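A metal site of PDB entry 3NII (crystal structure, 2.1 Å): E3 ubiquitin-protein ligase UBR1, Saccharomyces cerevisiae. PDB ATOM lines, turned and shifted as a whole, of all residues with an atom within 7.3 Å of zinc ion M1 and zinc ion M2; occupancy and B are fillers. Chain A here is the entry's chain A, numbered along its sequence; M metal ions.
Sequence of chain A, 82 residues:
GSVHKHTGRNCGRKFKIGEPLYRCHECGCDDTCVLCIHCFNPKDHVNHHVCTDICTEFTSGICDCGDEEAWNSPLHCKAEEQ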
ATOM      1  N   HIS A   4      18.637  31.986  10.129  1.00  0.00           N
ATOM      2  CA  HIS A   4      17.799  31.108   9.303  1.00  0.00           C
ATOM      3  C   HIS A   4      16.395  31.663   9.079  1.00  0.00           C
ATOM      4  O   HIS A   4      15.530  30.991   8.501  1.00  0.00           O
ATOM      5  CB  HIS A   4      17.726  29.713   9.922  1.00  0.00           C
ATOM      6  CG  HIS A   4      18.855  29.392  10.844  1.00  0.00           C
ATOM      7  ND1 HIS A   4      20.101  29.012  10.389  1.00  0.00           N
ATOM      8  CD2 HIS A   4      18.933  29.393  12.194  1.00  0.00           C
ATOM      9  CE1 HIS A   4      20.904  28.796  11.416  1.00  0.00           C
ATOM     10  NE2 HIS A   4      20.220  29.017  12.532  1.00  0.00           N
ATOM     11  N   LYS A   5      16.179  32.903   9.525  1.00  0.00           N
ATOM     12  CA  LYS A   5      14.921  33.623   9.300  1.00  0.00           C
ATOM     13  C   LYS A   5      14.677  33.799   7.815  1.00  0.00           C
ATOM     14  O   LYS A   5      15.620  33.969   7.026  1.00  0.00           O
ATOM     15  CB  LYS A   5      14.971  35.004   9.971  1.00  0.00           C
ATOM     16  CG  LYS A   5      15.150  34.974  11.483  1.00  0.00           C
ATOM     17  CD  LYS A   5      15.286  36.377  12.056  1.00  0.00           C
ATOM     18  CE  LYS A   5      15.495  36.331  13.565  1.00  0.00           C
ATOM     19  NZ  LYS A   5      15.634  37.693  14.153  1.00  0.00           N
ATOM     20  N   HIS A   6      13.411  33.751   7.416  1.00  0.00           N
ATOM     21  CA  HIS A   6      13.018  33.898   6.011  1.00  0.00           C
ATOM     22  C   HIS A   6      11.673  34.619   5.894  1.00  0.00           C
ATOM     23  O   HIS A   6      10.841  34.263   5.055  1.00  0.00           O
ATOM     24  CB  HIS A   6      12.987  32.529   5.319  1.00  0.00           C
ATOM     25  CG  HIS A   6      12.000  31.579   5.906  1.00  0.00           C
ATOM     26  ND1 HIS A   6      10.685  31.512   5.496  1.00  0.00           N
ATOM     27  CD2 HIS A   6      12.132  30.657   6.896  1.00  0.00           C
ATOM     28  CE1 HIS A   6      10.064  30.587   6.191  1.00  0.00           C
ATOM     29  NE2 HIS A   6      10.911  30.052   7.041  1.00  0.00           N
ATOM     30  N   THR A   7      11.483  35.632   6.733  1.00  0.00           N
ATOM     31  CA  THR A   7      10.249  36.427   6.780  1.00  0.00           C
ATOM     32  C   THR A   7       9.711  36.762   5.389  1.00  0.00           C
ATOM     33  O   THR A   7      10.425  37.288   4.543  1.00  0.00           O
ATOM     34  CB  THR A   7      10.479  37.749   7.570  1.00  0.00           C
ATOM     35  OG1 THR A   7      11.278  37.485   8.734  1.00  0.00           O
ATOM     36  CG2 THR A   7       9.154  38.375   7.987  1.00  0.00           C
ATOM     37  N   ARG A   9       8.566  34.790   2.941  1.00  0.00           N
ATOM     38  CA  ARG A   9       8.724  33.780   1.886  1.00  0.00           C
ATOM     39  C   ARG A   9       8.918  32.394   2.482  1.00  0.00           C
ATOM     40  O   ARG A   9       8.976  32.238   3.708  1.00  0.00           O
ATOM     41  CB  ARG A   9       9.866  34.144   0.912  1.00  0.00           C
ATOM     42  CG  ARG A   9      11.191  34.529   1.581  1.00  0.00           C
ATOM     43  CD  ARG A   9      12.390  34.202   0.702  1.00  0.00           C
ATOM     44  NE  ARG A   9      12.691  32.770   0.721  1.00  0.00           N
ATOM     45  CZ  ARG A   9      13.819  32.233   0.274  1.00  0.00           C
ATOM     46  NH1 ARG A   9      14.778  32.993  -0.238  1.00  0.00           N
ATOM     47  NH2 ARG A   9      13.988  30.919   0.339  1.00  0.00           N
ATOM     48  N   ASN A  10       8.987  31.381   1.621  1.00  0.00           N
ATOM     49  CA  ASN A  10       9.207  30.011   2.065  1.00  0.00           C
ATOM     50  C   ASN A  10      10.654  29.815   2.546  1.00  0.00           C
ATOM     51  O   ASN A  10      11.556  30.572   2.155  1.00  0.00           O
ATOM     52  CB  ASN A  10       8.904  29.033   0.915  1.00  0.00           C
ATOM     53  CG  ASN A  10       9.927  29.096  -0.199  1.00  0.00           C
ATOM     54  OD1 ASN A  10      10.120  30.144  -0.823  1.00  0.00           O
ATOM     55  ND2 ASN A  10      10.593  27.982  -0.471  1.00  0.00           N
ATOM     56  N   CYS A  11      10.868  28.812   3.396  1.00  0.00           N
ATOM     57  CA  CYS A  11      12.222  28.486   3.843  1.00  0.00           C
ATOM     58  C   CYS A  11      13.023  27.904   2.671  1.00  0.00           C
ATOM     59  O   CYS A  11      13.986  28.517   2.204  1.00  0.00           O
ATOM     60  CB  CYS A  11      12.196  27.529   5.036  1.00  0.00           C
ATOM     61  SG  CYS A  11      13.847  27.084   5.624  1.00  0.00           S
ATOM     62  N   GLY A  12      12.596  26.741   2.198  1.00  0.00           N
ATOM     63  CA  GLY A  12      13.254  26.092   1.059  1.00  0.00           C
ATOM     64  C   GLY A  12      14.634  25.526   1.350  1.00  0.00           C
ATOM     65  O   GLY A  12      15.327  25.081   0.436  1.00  0.00           O
ATOM     66  N   ARG A  13      15.047  25.543   2.626  1.00  0.00           N
ATOM     67  CA  ARG A  13      16.322  24.953   3.052  1.00  0.00           C
ATOM     68  C   ARG A  13      16.376  23.488   2.658  1.00  0.00           C
ATOM     69  O   ARG A  13      15.534  22.699   3.068  1.00  0.00           O
ATOM     70  CB  ARG A  13      16.513  25.102   4.567  1.00  0.00           C
ATOM     71  CG  ARG A  13      17.753  24.388   5.133  1.00  0.00           C
ATOM     72  CD  ARG A  13      17.888  24.628   6.627  1.00  0.00           C
ATOM     73  NE  ARG A  13      18.672  25.821   6.885  1.00  0.00           N
ATOM     74  CZ  ARG A  13      19.988  25.817   7.091  1.00  0.00           C
ATOM     75  NH1 ARG A  13      20.662  24.667   7.091  1.00  0.00           N
ATOM     76  NH2 ARG A  13      20.637  26.959   7.301  1.00  0.00           N
ATOM     77  N   PHE A  15      17.625  19.742   2.726  1.00  0.00           N
ATOM     78  CA  PHE A  15      18.148  18.818   3.723  1.00  0.00           C
ATOM     79  C   PHE A  15      19.383  18.075   3.228  1.00  0.00           C
ATOM     80  O   PHE A  15      19.489  17.745   2.048  1.00  0.00           O
ATOM     81  CB  PHE A  15      17.078  17.801   4.152  1.00  0.00           C
ATOM     82  CG  PHE A  15      15.911  18.415   4.870  1.00  0.00           C
ATOM     83  CD1 PHE A  15      15.982  18.675   6.246  1.00  0.00           C
ATOM     84  CD2 PHE A  15      14.745  18.728   4.192  1.00  0.00           C
ATOM     85  CE1 PHE A  15      14.900  19.245   6.908  1.00  0.00           C
ATOM     86  CE2 PHE A  15      13.655  19.303   4.851  1.00  0.00           C
ATOM     87  CZ  PHE A  15      13.725  19.564   6.202  1.00  0.00           C
ATOM     88  N   VAL A  34       7.305  18.945   5.100  1.00  0.00           N
ATOM     89  CA  VAL A  34       8.357  18.847   6.119  1.00  0.00           C
ATOM     90  C   VAL A  34       8.883  20.187   6.631  1.00  0.00           C
ATOM     91  O   VAL A  34       8.776  21.210   5.956  1.00  0.00           O
ATOM     92  CB  VAL A  34       9.583  18.017   5.620  1.00  0.00           C
ATOM     93  CG1 VAL A  34       9.207  16.560   5.405  1.00  0.00           C
ATOM     94  CG2 VAL A  34      10.158  18.591   4.342  1.00  0.00           C
ATOM     95  N   LEU A  35       9.471  20.159   7.826  1.00  0.00           N
ATOM     96  CA  LEU A  35      10.104  21.321   8.426  1.00  0.00           C
ATOM     97  C   LEU A  35      11.528  20.978   8.836  1.00  0.00           C
ATOM     98  O   LEU A  35      11.797  19.849   9.243  1.00  0.00           O
ATOM     99  CB  LEU A  35       9.327  21.792   9.657  1.00  0.00           C
ATOM    100  CG  LEU A  35       7.891  22.275   9.443  1.00  0.00           C
ATOM    101  CD1 LEU A  35       7.083  22.203  10.737  1.00  0.00           C
ATOM    102  CD2 LEU A  35       7.881  23.698   8.880  1.00  0.00           C
ATOM    103  N   CYS A  36      12.432  21.941   8.716  1.00  0.00           N
ATOM    104  CA  CYS A  36      13.800  21.787   9.207  1.00  0.00           C
ATOM    105  C   CYS A  36      13.866  22.110  10.696  1.00  0.00           C
ATOM    106  O   CYS A  36      12.908  22.645  11.261  1.00  0.00           O
ATOM    107  CB  CYS A  36      14.773  22.665   8.417  1.00  0.00           C
ATOM    108  SG  CYS A  36      14.693  24.438   8.782  1.00  0.00           S
ATOM    109  N   ILE A  37      15.014  21.823  11.312  1.00  0.00           N
ATOM    110  CA  ILE A  37      15.211  22.040  12.748  1.00  0.00           C
ATOM    111  C   ILE A  37      15.147  23.535  13.124  1.00  0.00           C
ATOM    112  O   ILE A  37      14.702  23.886  14.212  1.00  0.00           O
ATOM    113  CB  ILE A  37      16.519  21.348  13.286  1.00  0.00           C
ATOM    114  CG1 ILE A  37      16.512  21.255  14.817  1.00  0.00           C
ATOM    115  CG2 ILE A  37      17.784  22.046  12.726  1.00  0.00           C
ATOM    116  CD1 ILE A  37      17.467  20.211  15.420  1.00  0.00           C
ATOM    117  N   HIS A  38      15.561  24.401  12.208  1.00  0.00           N
ATOM    118  CA  HIS A  38      15.551  25.841  12.464  1.00  0.00           C
ATOM    119  C   HIS A  38      14.138  26.434  12.405  1.00  0.00           C
ATOM    120  O   HIS A  38      13.888  27.504  12.972  1.00  0.00           O
ATOM    121  CB  HIS A  38      16.473  26.564  11.477  1.00  0.00           C
ATOM    122  CG  HIS A  38      17.842  25.965  11.386  1.00  0.00           C
ATOM    123  ND1 HIS A  38      18.615  25.725  12.499  1.00  0.00           N
ATOM    124  CD2 HIS A  38      18.561  25.552  10.321  1.00  0.00           C
ATOM    125  CE1 HIS A  38      19.761  25.186  12.125  1.00  0.00           C
ATOM    126  NE2 HIS A  38      19.755  25.071  10.810  1.00  0.00           N
ATOM    127  N   CYS A  39      13.223  25.717  11.751  1.00  0.00           N
ATOM    128  CA  CYS A  39      11.864  26.206  11.521  1.00  0.00           C
ATOM    129  C   CYS A  39      10.828  25.560  12.448  1.00  0.00           C
ATOM    130  O   CYS A  39       9.915  26.240  12.943  1.00  0.00           O
ATOM    131  CB  CYS A  39      11.467  25.985  10.054  1.00  0.00           C
ATOM    132  SG  CYS A  39      12.329  27.019   8.799  1.00  0.00           S
ATOM    133  N   PHE A  40      10.956  24.253  12.675  1.00  0.00           N
ATOM    134  CA  PHE A  40      10.014  23.512  13.531  1.00  0.00           C
ATOM    135  C   PHE A  40       9.888  24.143  14.922  1.00  0.00           C
ATOM    136  O   PHE A  40      10.877  24.258  15.663  1.00  0.00           O
ATOM    137  CB  PHE A  40      10.407  22.046  13.642  1.00  0.00           C
ATOM    138  CG  PHE A  40       9.485  21.224  14.526  1.00  0.00           C
ATOM    139  CD1 PHE A  40       8.296  20.710  14.018  1.00  0.00           C
ATOM    140  CD2 PHE A  40       9.824  20.956  15.853  1.00  0.00           C
ATOM    141  CE1 PHE A  40       7.445  19.942  14.831  1.00  0.00           C
ATOM    142  CE2 PHE A  40       8.980  20.199  16.671  1.00  0.00           C
ATOM    143  CZ  PHE A  40       7.790  19.698  16.156  1.00  0.00           C
ATOM    144  N   ILE A  62      13.285  19.684   0.616  1.00  0.00           N
ATOM    145  CA  ILE A  62      13.409  21.029   1.179  1.00  0.00           C
ATOM    146  C   ILE A  62      12.340  21.331   2.226  1.00  0.00           C
ATOM    147  O   ILE A  62      11.268  20.735   2.232  1.00  0.00           O
ATOM    148  CB  ILE A  62      13.374  22.135   0.070  1.00  0.00           C
ATOM    149  CG1 ILE A  62      12.054  22.068  -0.708  1.00  0.00           C
ATOM    150  CG2 ILE A  62      14.567  21.997  -0.869  1.00  0.00           C
ATOM    151  CD1 ILE A  62      11.615  23.399  -1.289  1.00  0.00           C
ATOM    152  N   CYS A  63      12.652  22.277   3.100  1.00  0.00           N
ATOM    153  CA  CYS A  63      11.755  22.697   4.164  1.00  0.00           C
ATOM    154  C   CYS A  63      10.568  23.473   3.581  1.00  0.00           C
ATOM    155  O   CYS A  63      10.751  24.308   2.689  1.00  0.00           O
ATOM    156  CB  CYS A  63      12.517  23.562   5.165  1.00  0.00           C
ATOM    157  SG  CYS A  63      11.507  24.219   6.483  1.00  0.00           S
ATOM    158  N   ASP A  64       9.377  23.175   4.099  1.00  0.00           N
ATOM    159  CA  ASP A  64       8.134  23.770   3.610  1.00  0.00           C
ATOM    160  C   ASP A  64       7.611  24.915   4.465  1.00  0.00           C
ATOM    161  O   ASP A  64       6.532  25.443   4.205  1.00  0.00           O
ATOM    162  CB  ASP A  64       7.065  22.691   3.438  1.00  0.00           C
ATOM    163  CG  ASP A  64       7.463  21.627   2.437  1.00  0.00           C
ATOM    164  OD1 ASP A  64       7.823  22.003   1.314  1.00  0.00           O
ATOM    165  OD2 ASP A  64       7.456  20.428   2.787  1.00  0.00           O
ATOM    166  N   CYS A  65       8.374  25.293   5.493  1.00  0.00           N
ATOM    167  CA  CYS A  65       7.987  26.410   6.352  1.00  0.00           C
ATOM    168  C   CYS A  65       7.767  27.673   5.526  1.00  0.00           C
ATOM    169  O   CYS A  65       8.604  28.036   4.699  1.00  0.00           O
ATOM    170  CB  CYS A  65       9.042  26.669   7.415  1.00  0.00           C
ATOM    171  SG  CYS A  65       8.545  27.865   8.677  1.00  0.00           S
ATOM    172  N   GLY A  66       6.635  28.336   5.750  1.00  0.00           N
ATOM    173  CA  GLY A  66       6.295  29.541   5.011  1.00  0.00           C
ATOM    174  C   GLY A  66       5.588  29.296   3.695  1.00  0.00           C
ATOM    175  O   GLY A  66       5.118  30.241   3.053  1.00  0.00           O
ATOM    176  N   HIS A  76       4.383  29.100  13.154  1.00  0.00           N
ATOM    177  CA  HIS A  76       5.179  30.204  13.682  1.00  0.00           C
ATOM    178  C   HIS A  76       6.643  29.800  13.726  1.00  0.00           C
ATOM    179  O   HIS A  76       7.097  29.180  14.695  1.00  0.00           O
ATOM    180  CB  HIS A  76       4.682  30.613  15.066  1.00  0.00           C
ATOM    181  CG  HIS A  76       3.204  30.855  15.138  1.00  0.00           C
ATOM    182  ND1 HIS A  76       2.305  29.870  15.473  1.00  0.00           N
ATOM    183  CD2 HIS A  76       2.476  31.969  14.878  1.00  0.00           C
ATOM    184  CE1 HIS A  76       1.077  30.367  15.436  1.00  0.00           C
ATOM    185  NE2 HIS A  76       1.157  31.645  15.082  1.00  0.00           N
ATOM    186  N   CYS A  77       7.369  30.152  12.659  1.00  0.00           N
ATOM    187  CA  CYS A  77       8.769  29.797  12.459  1.00  0.00           C
ATOM    188  C   CYS A  77       9.599  29.969  13.735  1.00  0.00           C
ATOM    189  O   CYS A  77       9.558  31.024  14.368  1.00  0.00           O
ATOM    190  CB  CYS A  77       9.371  30.644  11.328  1.00  0.00           C
ATOM    191  SG  CYS A  77      10.856  29.976  10.519  1.00  0.00           S
ATOM    192  N   LYS A  78      10.336  28.919  14.109  1.00  0.00           N
ATOM    193  CA  LYS A  78      11.217  28.972  15.283  1.00  0.00           C
ATOM    194  C   LYS A  78      12.402  29.925  15.082  1.00  0.00           C
ATOM    195  O   LYS A  78      12.840  30.585  16.030  1.00  0.00           O
ATOM    196  CB  LYS A  78      11.720  27.579  15.677  1.00  0.00           C
ATOM    197  CG  LYS A  78      12.240  27.500  17.119  1.00  0.00           C
ATOM    198  CD  LYS A  78      13.000  26.202  17.389  1.00  0.00           C
ATOM    199  CE  LYS A  78      14.470  26.301  16.981  1.00  0.00           C
ATOM    200  NZ  LYS A  78      15.289  27.047  17.986  1.00  0.00           N
ATOM    201  N   ALA A  79      12.908  30.002  13.850  1.00  0.00           N
ATOM    202  CA  ALA A  79      13.986  30.933  13.499  1.00  0.00           C
ATOM    203  C   ALA A  79      13.585  32.387  13.765  1.00  0.00           C
ATOM    204  O   ALA A  79      14.414  33.224  14.106  1.00  0.00           O
ATOM    205  CB  ALA A  79      14.410  30.750  12.055  1.00  0.00           C
ATOM    206  N   GLU A  80      12.285  32.660  13.611  1.00  0.00           N
ATOM    207  CA  GLU A  80      11.705  33.985  13.831  1.00  0.00           C
ATOM    208  C   GLU A  80      11.662  34.360  15.325  1.00  0.00           C
ATOM    209  O   GLU A  80      11.278  35.479  15.684  1.00  0.00           O
ATOM    210  CB  GLU A  80      10.301  34.033  13.219  1.00  0.00           C
ATOM    211  CG  GLU A  80       9.831  35.414  12.760  1.00  0.00           C
ATOM    212  CD  GLU A  80      10.404  35.830  11.406  1.00  0.00           C
ATOM    213  OE1 GLU A  80      11.052  35.013  10.718  1.00  0.00           O
ATOM    214  OE2 GLU A  80      10.191  37.006  11.039  1.00  0.00           O
HETATM  215 ZN    ZN M   1      10.801  28.752   8.975  1.00  0.00          ZN
HETATM  216 ZN    ZN M   2      13.121  25.615   7.392  1.00  0.00          ZN
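O of Arg 13 lies within hydrogen-bond range of N of Cys 63 (2.9 Å). O of Cys 39 lies within hydrogen-bond range of N of Lys 78. The side-chain sulfur (SG) of Cys 11 sits close to the backbone NH (N) of Arg 13 (3.6 Å). A ring nitrogen (ND1) of His 6 lies close to the backbone NH (N) of Cys 11 (3.4 Å). The side-chain sulfur (SG) of Cys 36 lies close to the backbone NH (N) of His 38 (3.5 Å). The backbone carbonyl oxygen of Cys 11 lies within hydrogen-bond range of the guanidinium group of Arg 9 (3.0 Å). The backbone carbonyl oxygen of Cys 63 is in hydrogen-bond range of the backbone NH of Gly 12, 3.1 Å away. The backbone NH (N) of Cys 11 lies within hydrogen-bond range of the backbone carbonyl oxygen (O) of Cys 65, at 2.7 Å.
Four residues have an atom within 4 Å of zinc ion M1: His 6, Cys 39, Cys 65 and Cys 77.
Of the 27 residues printed, 4 come within 4 Å of zinc ion M2. The nearest printed residue that does not touch zinc ion M2 is Cys 65 (4.2 Å).
SG of Cys 77 binds zinc ion M1 (2.0 Å). Zinc ion M1 is bound by SG of Cys 39, 2.3 Å away. NE2 of His 6 binds zinc ion M1 (2.3 Å). Zinc ion M1 is bound by the side-chain sulfur (SG) of Cys 65, at 2.4 Å. Zinc ion M1 has four donor atoms within binding distance.
Zinc ion M2 is bound by SG of Cys 39, SG of Cys 63, SG of Cys 36 and SG of Cys 11. Zinc ion M2 has four donor atoms within binding distance.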
